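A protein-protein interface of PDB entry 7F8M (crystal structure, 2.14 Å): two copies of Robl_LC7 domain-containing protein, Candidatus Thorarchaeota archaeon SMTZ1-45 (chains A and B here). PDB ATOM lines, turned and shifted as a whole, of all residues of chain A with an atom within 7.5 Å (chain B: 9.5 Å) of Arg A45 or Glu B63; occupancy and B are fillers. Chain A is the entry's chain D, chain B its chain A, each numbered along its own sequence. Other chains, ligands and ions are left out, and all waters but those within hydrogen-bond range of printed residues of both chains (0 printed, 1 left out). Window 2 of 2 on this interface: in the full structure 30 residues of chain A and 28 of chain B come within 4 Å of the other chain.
The backbone carbonyl oxygen of Glu B63 is in hydrogen-bond range of the guanidinium group of Arg A45, 2.6 Å away.
NZ of Lys B59 lies within salt-bridge range of OE1 of Glu B63 (2.9 Å). N of Arg B66 is in hydrogen-bond range of O of Thr B61, at 3.1 Å. O of Leu B64 lies within hydrogen-bond range of NE of Arg B66 (3.2 Å).
Val A46 touches Leu B64 (CG2 to CD2, 3.9 Å). Ile A49 touches Glu B63. Leu B64 touches Ile A49 (CG to CG2, 3.8 Å). Ala B60 touches Leu A53 (CB to CD2, 3.7 Å). Thr A81 touches Leu B64. OG1 of Thr A81 touches CG of Arg B66 (3.2 Å).
No position is printed for both chains.
Of chain B, only Glu B63 (2.6 Å) comes within 4 Å of Arg A45. No residue of chain B comes within 4 Å of Ala A48. Of chain B, only Glu B63 (3.7 Å) and Leu B64 (3.8 Å) come within 4 Å of Ile A49. Of the printed residues of chain B, Leu A53 touches Ala B60 (3.7 Å). Of the printed residues of chain B, Thr A81 touches Leu B64 (3.6 Å) and Arg B66 (3.2 Å). Of chain A, only Arg A45 and Ile A49 come within 4 Å of Glu B63. Of the printed residues of chain A, Leu B64 touches Val A46, Ile A49 and Thr A81. Printed residues of chain A within 4 Å of Arg B66: Thr A81 (3.2 Å). The nearest residue of chain B that does not touch Arg A45 is Leu B64 (4.5 Å). The nearest residue of chain A that does not touch Glu B63 is Val A46 (6.0 Å).
Of the 14 printed residues of chain B, 4 touch a printed residue of chain A. Hydrophobic or aromatic side chains of chain B within 4 Å of the printed part of chain A: Ala B60 and Leu B64. Along chain B the printed residues that touch a printed residue of chain A span positions 60 to 66. Of the 16 printed residues of chain A, 5 touch a printed residue of chain B. Among the printed residues, no Asp or Glu carboxylate lies within 4 Å of a Lys or Arg side-chain nitrogen of the other chain.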
ATOM      1  N   GLY A  31      -0.282   1.255 -11.366  1.00  0.00           N
ATOM      2  CA  GLY A  31       0.041   2.701 -11.401  1.00  0.00           C
ATOM      3  C   GLY A  31      -0.749   3.552 -12.395  1.00  0.00           C
ATOM      4  O   GLY A  31      -0.360   4.723 -12.576  1.00  0.00           O
ATOM      5  N   MET A  33      -4.126   5.654 -13.062  1.00  0.00           N
ATOM      6  CA  MET A  33      -5.249   6.425 -12.416  1.00  0.00           C
ATOM      7  C   MET A  33      -6.598   5.983 -12.993  1.00  0.00           C
ATOM      8  O   MET A  33      -6.702   5.782 -14.204  1.00  0.00           O
ATOM      9  CB  MET A  33      -5.075   7.933 -12.649  1.00  0.00           C
ATOM     10  CG  MET A  33      -6.191   8.825 -12.069  1.00  0.00           C
ATOM     11  SD  MET A  33      -6.333   8.730 -10.264  1.00  0.00           S
ATOM     12  CE  MET A  33      -4.920   9.681  -9.701  1.00  0.00           C
ATOM     13  N   THR A  41      -3.535  17.790 -14.214  1.00  0.00           N
ATOM     14  CA  THR A  41      -2.113  17.744 -14.654  1.00  0.00           C
ATOM     15  C   THR A  41      -1.308  16.787 -13.750  1.00  0.00           C
ATOM     16  O   THR A  41      -0.537  15.966 -14.303  1.00  0.00           O
ATOM     17  CB  THR A  41      -1.507  19.155 -14.703  1.00  0.00           C
ATOM     18  OG1 THR A  41      -0.135  18.989 -15.081  1.00  0.00           O
ATOM     19  CG2 THR A  41      -1.626  19.929 -13.402  1.00  0.00           C
ATOM     20  N   GLU A  42      -1.482  16.883 -12.424  1.00  0.00           N
ATOM     21  CA  GLU A  42      -0.722  16.126 -11.391  1.00  0.00           C
ATOM     22  C   GLU A  42      -1.170  14.653 -11.392  1.00  0.00           C
ATOM     23  O   GLU A  42      -0.375  13.803 -10.977  1.00  0.00           O
ATOM     24  CB  GLU A  42      -0.954  16.748 -10.003  1.00  0.00           C
ATOM     25  CG  GLU A  42      -0.538  18.215  -9.854  1.00  0.00           C
ATOM     26  CD  GLU A  42      -0.371  18.719  -8.413  1.00  0.00           C
ATOM     27  OE1 GLU A  42       0.399  19.672  -8.212  1.00  0.00           O
ATOM     28  OE2 GLU A  42      -1.009  18.170  -7.478  1.00  0.00           O
ATOM     29  N   GLN A  43      -2.412  14.366 -11.791  1.00  0.00           N
ATOM     30  CA  GLN A  43      -3.095  13.065 -11.539  1.00  0.00           C
ATOM     31  C   GLN A  43      -2.219  11.901 -12.025  1.00  0.00           C
ATOM     32  O   GLN A  43      -2.175  10.880 -11.332  1.00  0.00           O
ATOM     33  CB  GLN A  43      -4.489  13.006 -12.177  1.00  0.00           C
ATOM     34  CG  GLN A  43      -5.567  13.752 -11.390  1.00  0.00           C
ATOM     35  CD  GLN A  43      -6.929  13.632 -12.035  1.00  0.00           C
ATOM     36  OE1 GLN A  43      -7.240  12.673 -12.752  1.00  0.00           O
ATOM     37  NE2 GLN A  43      -7.754  14.638 -11.802  1.00  0.00           N
ATOM     38  N   GLU A  44      -1.547  12.028 -13.165  1.00  0.00           N
ATOM     39  CA  GLU A  44      -0.730  10.922 -13.737  1.00  0.00           C
ATOM     40  C   GLU A  44       0.474  10.646 -12.839  1.00  0.00           C
ATOM     41  O   GLU A  44       0.894   9.470 -12.780  1.00  0.00           O
ATOM     42  CB  GLU A  44      -0.249  11.261 -15.146  1.00  0.00           C
ATOM     43  CG  GLU A  44       0.313  10.069 -15.902  1.00  0.00           C
ATOM     44  CD  GLU A  44       0.567  10.376 -17.372  1.00  0.00           C
ATOM     45  OE1 GLU A  44       1.746  10.509 -17.711  1.00  0.00           O
ATOM     46  OE2 GLU A  44      -0.408  10.498 -18.167  1.00  0.00           O
ATOM     47  N   ARG A  45       1.028  11.705 -12.242  1.00  0.00           N
ATOM     48  CA  ARG A  45       2.220  11.663 -11.366  1.00  0.00           C
ATOM     49  C   ARG A  45       1.792  10.971 -10.060  1.00  0.00           C
ATOM     50  O   ARG A  45       2.393   9.954  -9.668  1.00  0.00           O
ATOM     51  CB  ARG A  45       2.772  13.079 -11.192  1.00  0.00           C
ATOM     52  CG  ARG A  45       4.074  13.150 -10.413  1.00  0.00           C
ATOM     53  CD  ARG A  45       4.429  14.539  -9.941  1.00  0.00           C
ATOM     54  NE  ARG A  45       3.570  15.060  -8.875  1.00  0.00           N
ATOM     55  CZ  ARG A  45       3.940  15.284  -7.595  1.00  0.00           C
ATOM     56  NH1 ARG A  45       5.162  14.995  -7.161  1.00  0.00           N
ATOM     57  NH2 ARG A  45       3.072  15.804  -6.737  1.00  0.00           N
ATOM     58  N   VAL A  46       0.697  11.432  -9.473  1.00  0.00           N
ATOM     59  CA  VAL A  46       0.178  11.019  -8.136  1.00  0.00           C
ATOM     60  C   VAL A  46      -0.210   9.532  -8.172  1.00  0.00           C
ATOM     61  O   VAL A  46      -0.103   8.861  -7.103  1.00  0.00           O
ATOM     62  CB  VAL A  46      -0.980  11.949  -7.732  1.00  0.00           C
ATOM     63  CG1 VAL A  46      -1.921  11.361  -6.678  1.00  0.00           C
ATOM     64  CG2 VAL A  46      -0.410  13.298  -7.297  1.00  0.00           C
ATOM     65  N   ALA A  47      -0.672   9.061  -9.334  1.00  0.00           N
ATOM     66  CA  ALA A  47      -0.954   7.636  -9.622  1.00  0.00           C
ATOM     67  C   ALA A  47       0.360   6.860  -9.552  1.00  0.00           C
ATOM     68  O   ALA A  47       0.326   5.711  -9.062  1.00  0.00           O
ATOM     69  CB  ALA A  47      -1.596   7.456 -10.973  1.00  0.00           C
ATOM     70  N   ALA A  48       1.467   7.444 -10.028  1.00  0.00           N
ATOM     71  CA  ALA A  48       2.799   6.799  -9.995  1.00  0.00           C
ATOM     72  C   ALA A  48       3.297   6.677  -8.562  1.00  0.00           C
ATOM     73  O   ALA A  48       3.785   5.583  -8.219  1.00  0.00           O
ATOM     74  CB  ALA A  48       3.802   7.508 -10.855  1.00  0.00           C
ATOM     75  N   ILE A  49       3.187   7.739  -7.762  1.00  0.00           N
ATOM     76  CA  ILE A  49       3.720   7.805  -6.363  1.00  0.00           C
ATOM     77  C   ILE A  49       2.968   6.805  -5.465  1.00  0.00           C
ATOM     78  O   ILE A  49       3.681   6.076  -4.740  1.00  0.00           O
ATOM     79  CB  ILE A  49       3.619   9.242  -5.825  1.00  0.00           C
ATOM     80  CG1 ILE A  49       4.452  10.208  -6.677  1.00  0.00           C
ATOM     81  CG2 ILE A  49       4.011   9.322  -4.368  1.00  0.00           C
ATOM     82  CD1 ILE A  49       4.004  11.663  -6.603  1.00  0.00           C
ATOM     83  N   SER A  50       1.620   6.707  -5.557  1.00  0.00           N
ATOM     84  CA  SER A  50       0.807   5.711  -4.813  1.00  0.00           C
ATOM     85  C   SER A  50       1.148   4.251  -5.167  1.00  0.00           C
ATOM     86  O   SER A  50       0.900   3.412  -4.280  1.00  0.00           O
ATOM     87  CB  SER A  50      -0.689   5.947  -4.949  1.00  0.00           C
ATOM     88  OG  SER A  50      -1.157   5.554  -6.233  1.00  0.00           O
ATOM     89  N   ALA A  51       1.648   3.965  -6.387  1.00  0.00           N
ATOM     90  CA  ALA A  51       2.250   2.698  -6.893  1.00  0.00           C
ATOM     91  C   ALA A  51       3.285   2.121  -5.950  1.00  0.00           C
ATOM     92  O   ALA A  51       3.198   0.906  -5.609  1.00  0.00           O
ATOM     93  CB  ALA A  51       2.958   2.881  -8.236  1.00  0.00           C
ATOM     94  N   GLY A  52       4.284   2.936  -5.650  1.00  0.00           N
ATOM     95  CA  GLY A  52       5.435   2.560  -4.823  1.00  0.00           C
ATOM     96  C   GLY A  52       5.015   2.423  -3.381  1.00  0.00           C
ATOM     97  O   GLY A  52       5.437   1.454  -2.714  1.00  0.00           O
ATOM     98  N   LEU A  53       4.174   3.316  -2.890  1.00  0.00           N
ATOM     99  CA  LEU A  53       3.711   3.217  -1.476  1.00  0.00           C
ATOM    100  C   LEU A  53       3.118   1.829  -1.168  1.00  0.00           C
ATOM    101  O   LEU A  53       3.277   1.349   0.009  1.00  0.00           O
ATOM    102  CB  LEU A  53       2.659   4.301  -1.217  1.00  0.00           C
ATOM    103  CG  LEU A  53       3.161   5.748  -1.304  1.00  0.00           C
ATOM    104  CD1 LEU A  53       2.172   6.651  -0.547  1.00  0.00           C
ATOM    105  CD2 LEU A  53       4.588   5.889  -0.752  1.00  0.00           C
ATOM    106  N   THR A  81      -0.552  11.329   4.249  1.00  0.00           N
ATOM    107  CA  THR A  81      -0.872  10.434   3.135  1.00  0.00           C
ATOM    108  C   THR A  81      -1.422   9.108   3.655  1.00  0.00           C
ATOM    109  O   THR A  81      -0.717   8.354   4.324  1.00  0.00           O
ATOM    110  CB  THR A  81       0.387  10.223   2.298  1.00  0.00           C
ATOM    111  OG1 THR A  81       0.861  11.458   1.757  1.00  0.00           O
ATOM    112  CG2 THR A  81       0.097   9.305   1.142  1.00  0.00           C
ATOM    113  N   SER B  55      13.175   5.632   4.579  1.00  0.00           N
ATOM    114  CA  SER B  55      13.514   6.242   3.267  1.00  0.00           C
ATOM    115  C   SER B  55      12.284   6.333   2.369  1.00  0.00           C
ATOM    116  O   SER B  55      12.168   7.322   1.629  1.00  0.00           O
ATOM    117  CB  SER B  55      14.623   5.477   2.600  1.00  0.00           C
ATOM    118  OG  SER B  55      15.700   5.301   3.512  1.00  0.00           O
ATOM    119  N   LEU B  56      11.348   5.396   2.479  1.00  0.00           N
ATOM    120  CA  LEU B  56      10.183   5.327   1.553  1.00  0.00           C
ATOM    121  C   LEU B  56       8.959   6.060   2.159  1.00  0.00           C
ATOM    122  O   LEU B  56       8.062   6.449   1.382  1.00  0.00           O
ATOM    123  CB  LEU B  56       9.936   3.855   1.201  1.00  0.00           C
ATOM    124  CG  LEU B  56      11.193   3.079   0.800  1.00  0.00           C
ATOM    125  CD1 LEU B  56      10.941   1.584   0.808  1.00  0.00           C
ATOM    126  CD2 LEU B  56      11.752   3.540  -0.539  1.00  0.00           C
ATOM    127  N   GLY B  57       8.959   6.321   3.471  1.00  0.00           N
ATOM    128  CA  GLY B  57       8.141   7.348   4.140  1.00  0.00           C
ATOM    129  C   GLY B  57       8.514   8.788   3.782  1.00  0.00           C
ATOM    130  O   GLY B  57       7.576   9.588   3.564  1.00  0.00           O
ATOM    131  N   GLU B  58       9.819   9.099   3.756  1.00  0.00           N
ATOM    132  CA  GLU B  58      10.436  10.325   3.173  1.00  0.00           C
ATOM    133  C   GLU B  58       9.886  10.564   1.772  1.00  0.00           C
ATOM    134  O   GLU B  58       9.460  11.694   1.508  1.00  0.00           O
ATOM    135  CB  GLU B  58      11.971  10.208   3.082  1.00  0.00           C
ATOM    136  CG  GLU B  58      12.705  10.392   4.415  1.00  0.00           C
ATOM    137  CD  GLU B  58      14.235  10.312   4.394  1.00  0.00           C
ATOM    138  OE1 GLU B  58      14.843  10.232   5.512  1.00  0.00           O
ATOM    139  OE2 GLU B  58      14.847  10.323   3.275  1.00  0.00           O
ATOM    140  N   LYS B  59       9.887   9.550   0.899  1.00  0.00           N
ATOM    141  CA  LYS B  59       9.410   9.699  -0.512  1.00  0.00           C
ATOM    142  C   LYS B  59       7.927  10.088  -0.539  1.00  0.00           C
ATOM    143  O   LYS B  59       7.558  11.033  -1.273  1.00  0.00           O
ATOM    144  CB  LYS B  59       9.614   8.425  -1.335  1.00  0.00           C
ATOM    145  CG  LYS B  59       8.361   7.630  -1.687  1.00  0.00           C
ATOM    146  CD  LYS B  59       8.690   6.250  -2.259  1.00  0.00           C
ATOM    147  CE  LYS B  59       9.434   6.319  -3.581  1.00  0.00           C
ATOM    148  NZ  LYS B  59       8.545   6.821  -4.642  1.00  0.00           N
ATOM    149  N   ALA B  60       7.101   9.417   0.260  1.00  0.00           N
ATOM    150  CA  ALA B  60       5.666   9.678   0.314  1.00  0.00           C
ATOM    151  C   ALA B  60       5.461  11.178   0.528  1.00  0.00           C
ATOM    152  O   ALA B  60       4.805  11.780  -0.349  1.00  0.00           O
ATOM    153  CB  ALA B  60       4.996   8.892   1.386  1.00  0.00           C
ATOM    154  N   THR B  61       6.070  11.727   1.589  1.00  0.00           N
ATOM    155  CA  THR B  61       5.845  13.090   2.137  1.00  0.00           C
ATOM    156  C   THR B  61       6.405  14.144   1.153  1.00  0.00           C
ATOM    157  O   THR B  61       5.678  15.011   0.715  1.00  0.00           O
ATOM    158  CB  THR B  61       6.312  13.112   3.606  1.00  0.00           C
ATOM    159  OG1 THR B  61       7.585  12.490   3.789  1.00  0.00           O
ATOM    160  CG2 THR B  61       5.380  12.367   4.550  1.00  0.00           C
ATOM    161  N   THR B  62       7.656  14.042   0.741  1.00  0.00           N
ATOM    162  CA  THR B  62       8.218  14.910  -0.316  1.00  0.00           C
ATOM    163  C   THR B  62       7.285  14.862  -1.535  1.00  0.00           C
ATOM    164  O   THR B  62       6.682  15.875  -1.891  1.00  0.00           O
ATOM    165  CB  THR B  62       9.656  14.480  -0.562  1.00  0.00           C
ATOM    166  OG1 THR B  62       9.538  13.113  -0.964  1.00  0.00           O
ATOM    167  CG2 THR B  62      10.514  14.643   0.684  1.00  0.00           C
ATOM    168  N   GLU B  63       7.056  13.693  -2.093  1.00  0.00           N
ATOM    169  CA  GLU B  63       6.533  13.603  -3.474  1.00  0.00           C
ATOM    170  C   GLU B  63       5.093  14.101  -3.568  1.00  0.00           C
ATOM    171  O   GLU B  63       4.783  14.634  -4.629  1.00  0.00           O
ATOM    172  CB  GLU B  63       6.673  12.178  -3.980  1.00  0.00           C
ATOM    173  CG  GLU B  63       8.098  11.825  -4.326  1.00  0.00           C
ATOM    174  CD  GLU B  63       8.186  10.708  -5.358  1.00  0.00           C
ATOM    175  OE1 GLU B  63       7.671   9.599  -5.052  1.00  0.00           O
ATOM    176  OE2 GLU B  63       8.715  10.960  -6.488  1.00  0.00           O
ATOM    177  N   LEU B  64       4.272  13.936  -2.519  1.00  0.00           N
ATOM    178  CA  LEU B  64       2.847  14.381  -2.453  1.00  0.00           C
ATOM    179  C   LEU B  64       2.675  15.684  -1.653  1.00  0.00           C
ATOM    180  O   LEU B  64       1.498  15.994  -1.319  1.00  0.00           O
ATOM    181  CB  LEU B  64       1.974  13.274  -1.839  1.00  0.00           C
ATOM    182  CG  LEU B  64       1.973  11.966  -2.623  1.00  0.00           C
ATOM    183  CD1 LEU B  64       1.410  10.840  -1.793  1.00  0.00           C
ATOM    184  CD2 LEU B  64       1.202  12.103  -3.927  1.00  0.00           C
ATOM    185  N   ASP B  65       3.743  16.444  -1.370  1.00  0.00           N
ATOM    186  CA  ASP B  65       3.608  17.815  -0.786  1.00  0.00           C
ATOM    187  C   ASP B  65       2.940  17.766   0.607  1.00  0.00           C
ATOM    188  O   ASP B  65       1.905  18.414   0.753  1.00  0.00           O
ATOM    189  CB  ASP B  65       2.786  18.685  -1.759  1.00  0.00           C
ATOM    190  CG  ASP B  65       2.837  20.187  -1.535  1.00  0.00           C
ATOM    191  OD1 ASP B  65       1.810  20.756  -1.089  1.00  0.00           O
ATOM    192  OD2 ASP B  65       3.887  20.780  -1.858  1.00  0.00           O
ATOM    193  N   ARG B  66       3.487  17.013   1.582  1.00  0.00           N
ATOM    194  CA  ARG B  66       2.838  16.755   2.907  1.00  0.00           C
ATOM    195  C   ARG B  66       3.643  17.317   4.087  1.00  0.00           C
ATOM    196  O   ARG B  66       3.134  17.148   5.236  1.00  0.00           O
ATOM    197  CB  ARG B  66       2.697  15.263   3.225  1.00  0.00           C
ATOM    198  CG  ARG B  66       1.843  14.454   2.267  1.00  0.00           C
ATOM    199  CD  ARG B  66       0.367  14.776   2.314  1.00  0.00           C
ATOM    200  NE  ARG B  66       0.025  15.905   1.471  1.00  0.00           N
ATOM    201  CZ  ARG B  66      -1.175  16.473   1.428  1.00  0.00           C
ATOM    202  NH1 ARG B  66      -1.376  17.509   0.632  1.00  0.00           N
ATOM    203  NH2 ARG B  66      -2.174  16.002   2.160  1.00  0.00           N
ATOM    204  N   GLY B  67       4.845  17.877   3.850  1.00  0.00           N
ATOM    205  CA  GLY B  67       5.721  18.458   4.887  1.00  0.00           C
ATOM    206  C   GLY B  67       6.789  17.497   5.344  1.00  0.00           C
ATOM    207  O   GLY B  67       6.755  16.326   4.888  1.00  0.00           O
ATOM    208  N   ASN B  68       7.656  17.949   6.263  1.00  0.00           N
ATOM    209  CA  ASN B  68       8.825  17.173   6.756  1.00  0.00           C
ATOM    210  C   ASN B  68       8.297  15.907   7.420  1.00  0.00           C
ATOM    211  O   ASN B  68       7.310  16.043   8.120  1.00  0.00           O
ATOM    212  CB  ASN B  68       9.746  17.979   7.679  1.00  0.00           C
ATOM    213  CG  ASN B  68      11.006  18.390   6.956  1.00  0.00           C
ATOM    214  OD1 ASN B  68      12.104  18.088   7.399  1.00  0.00           O
ATOM    215  ND2 ASN B  68      10.841  19.018   5.809  1.00  0.00           N
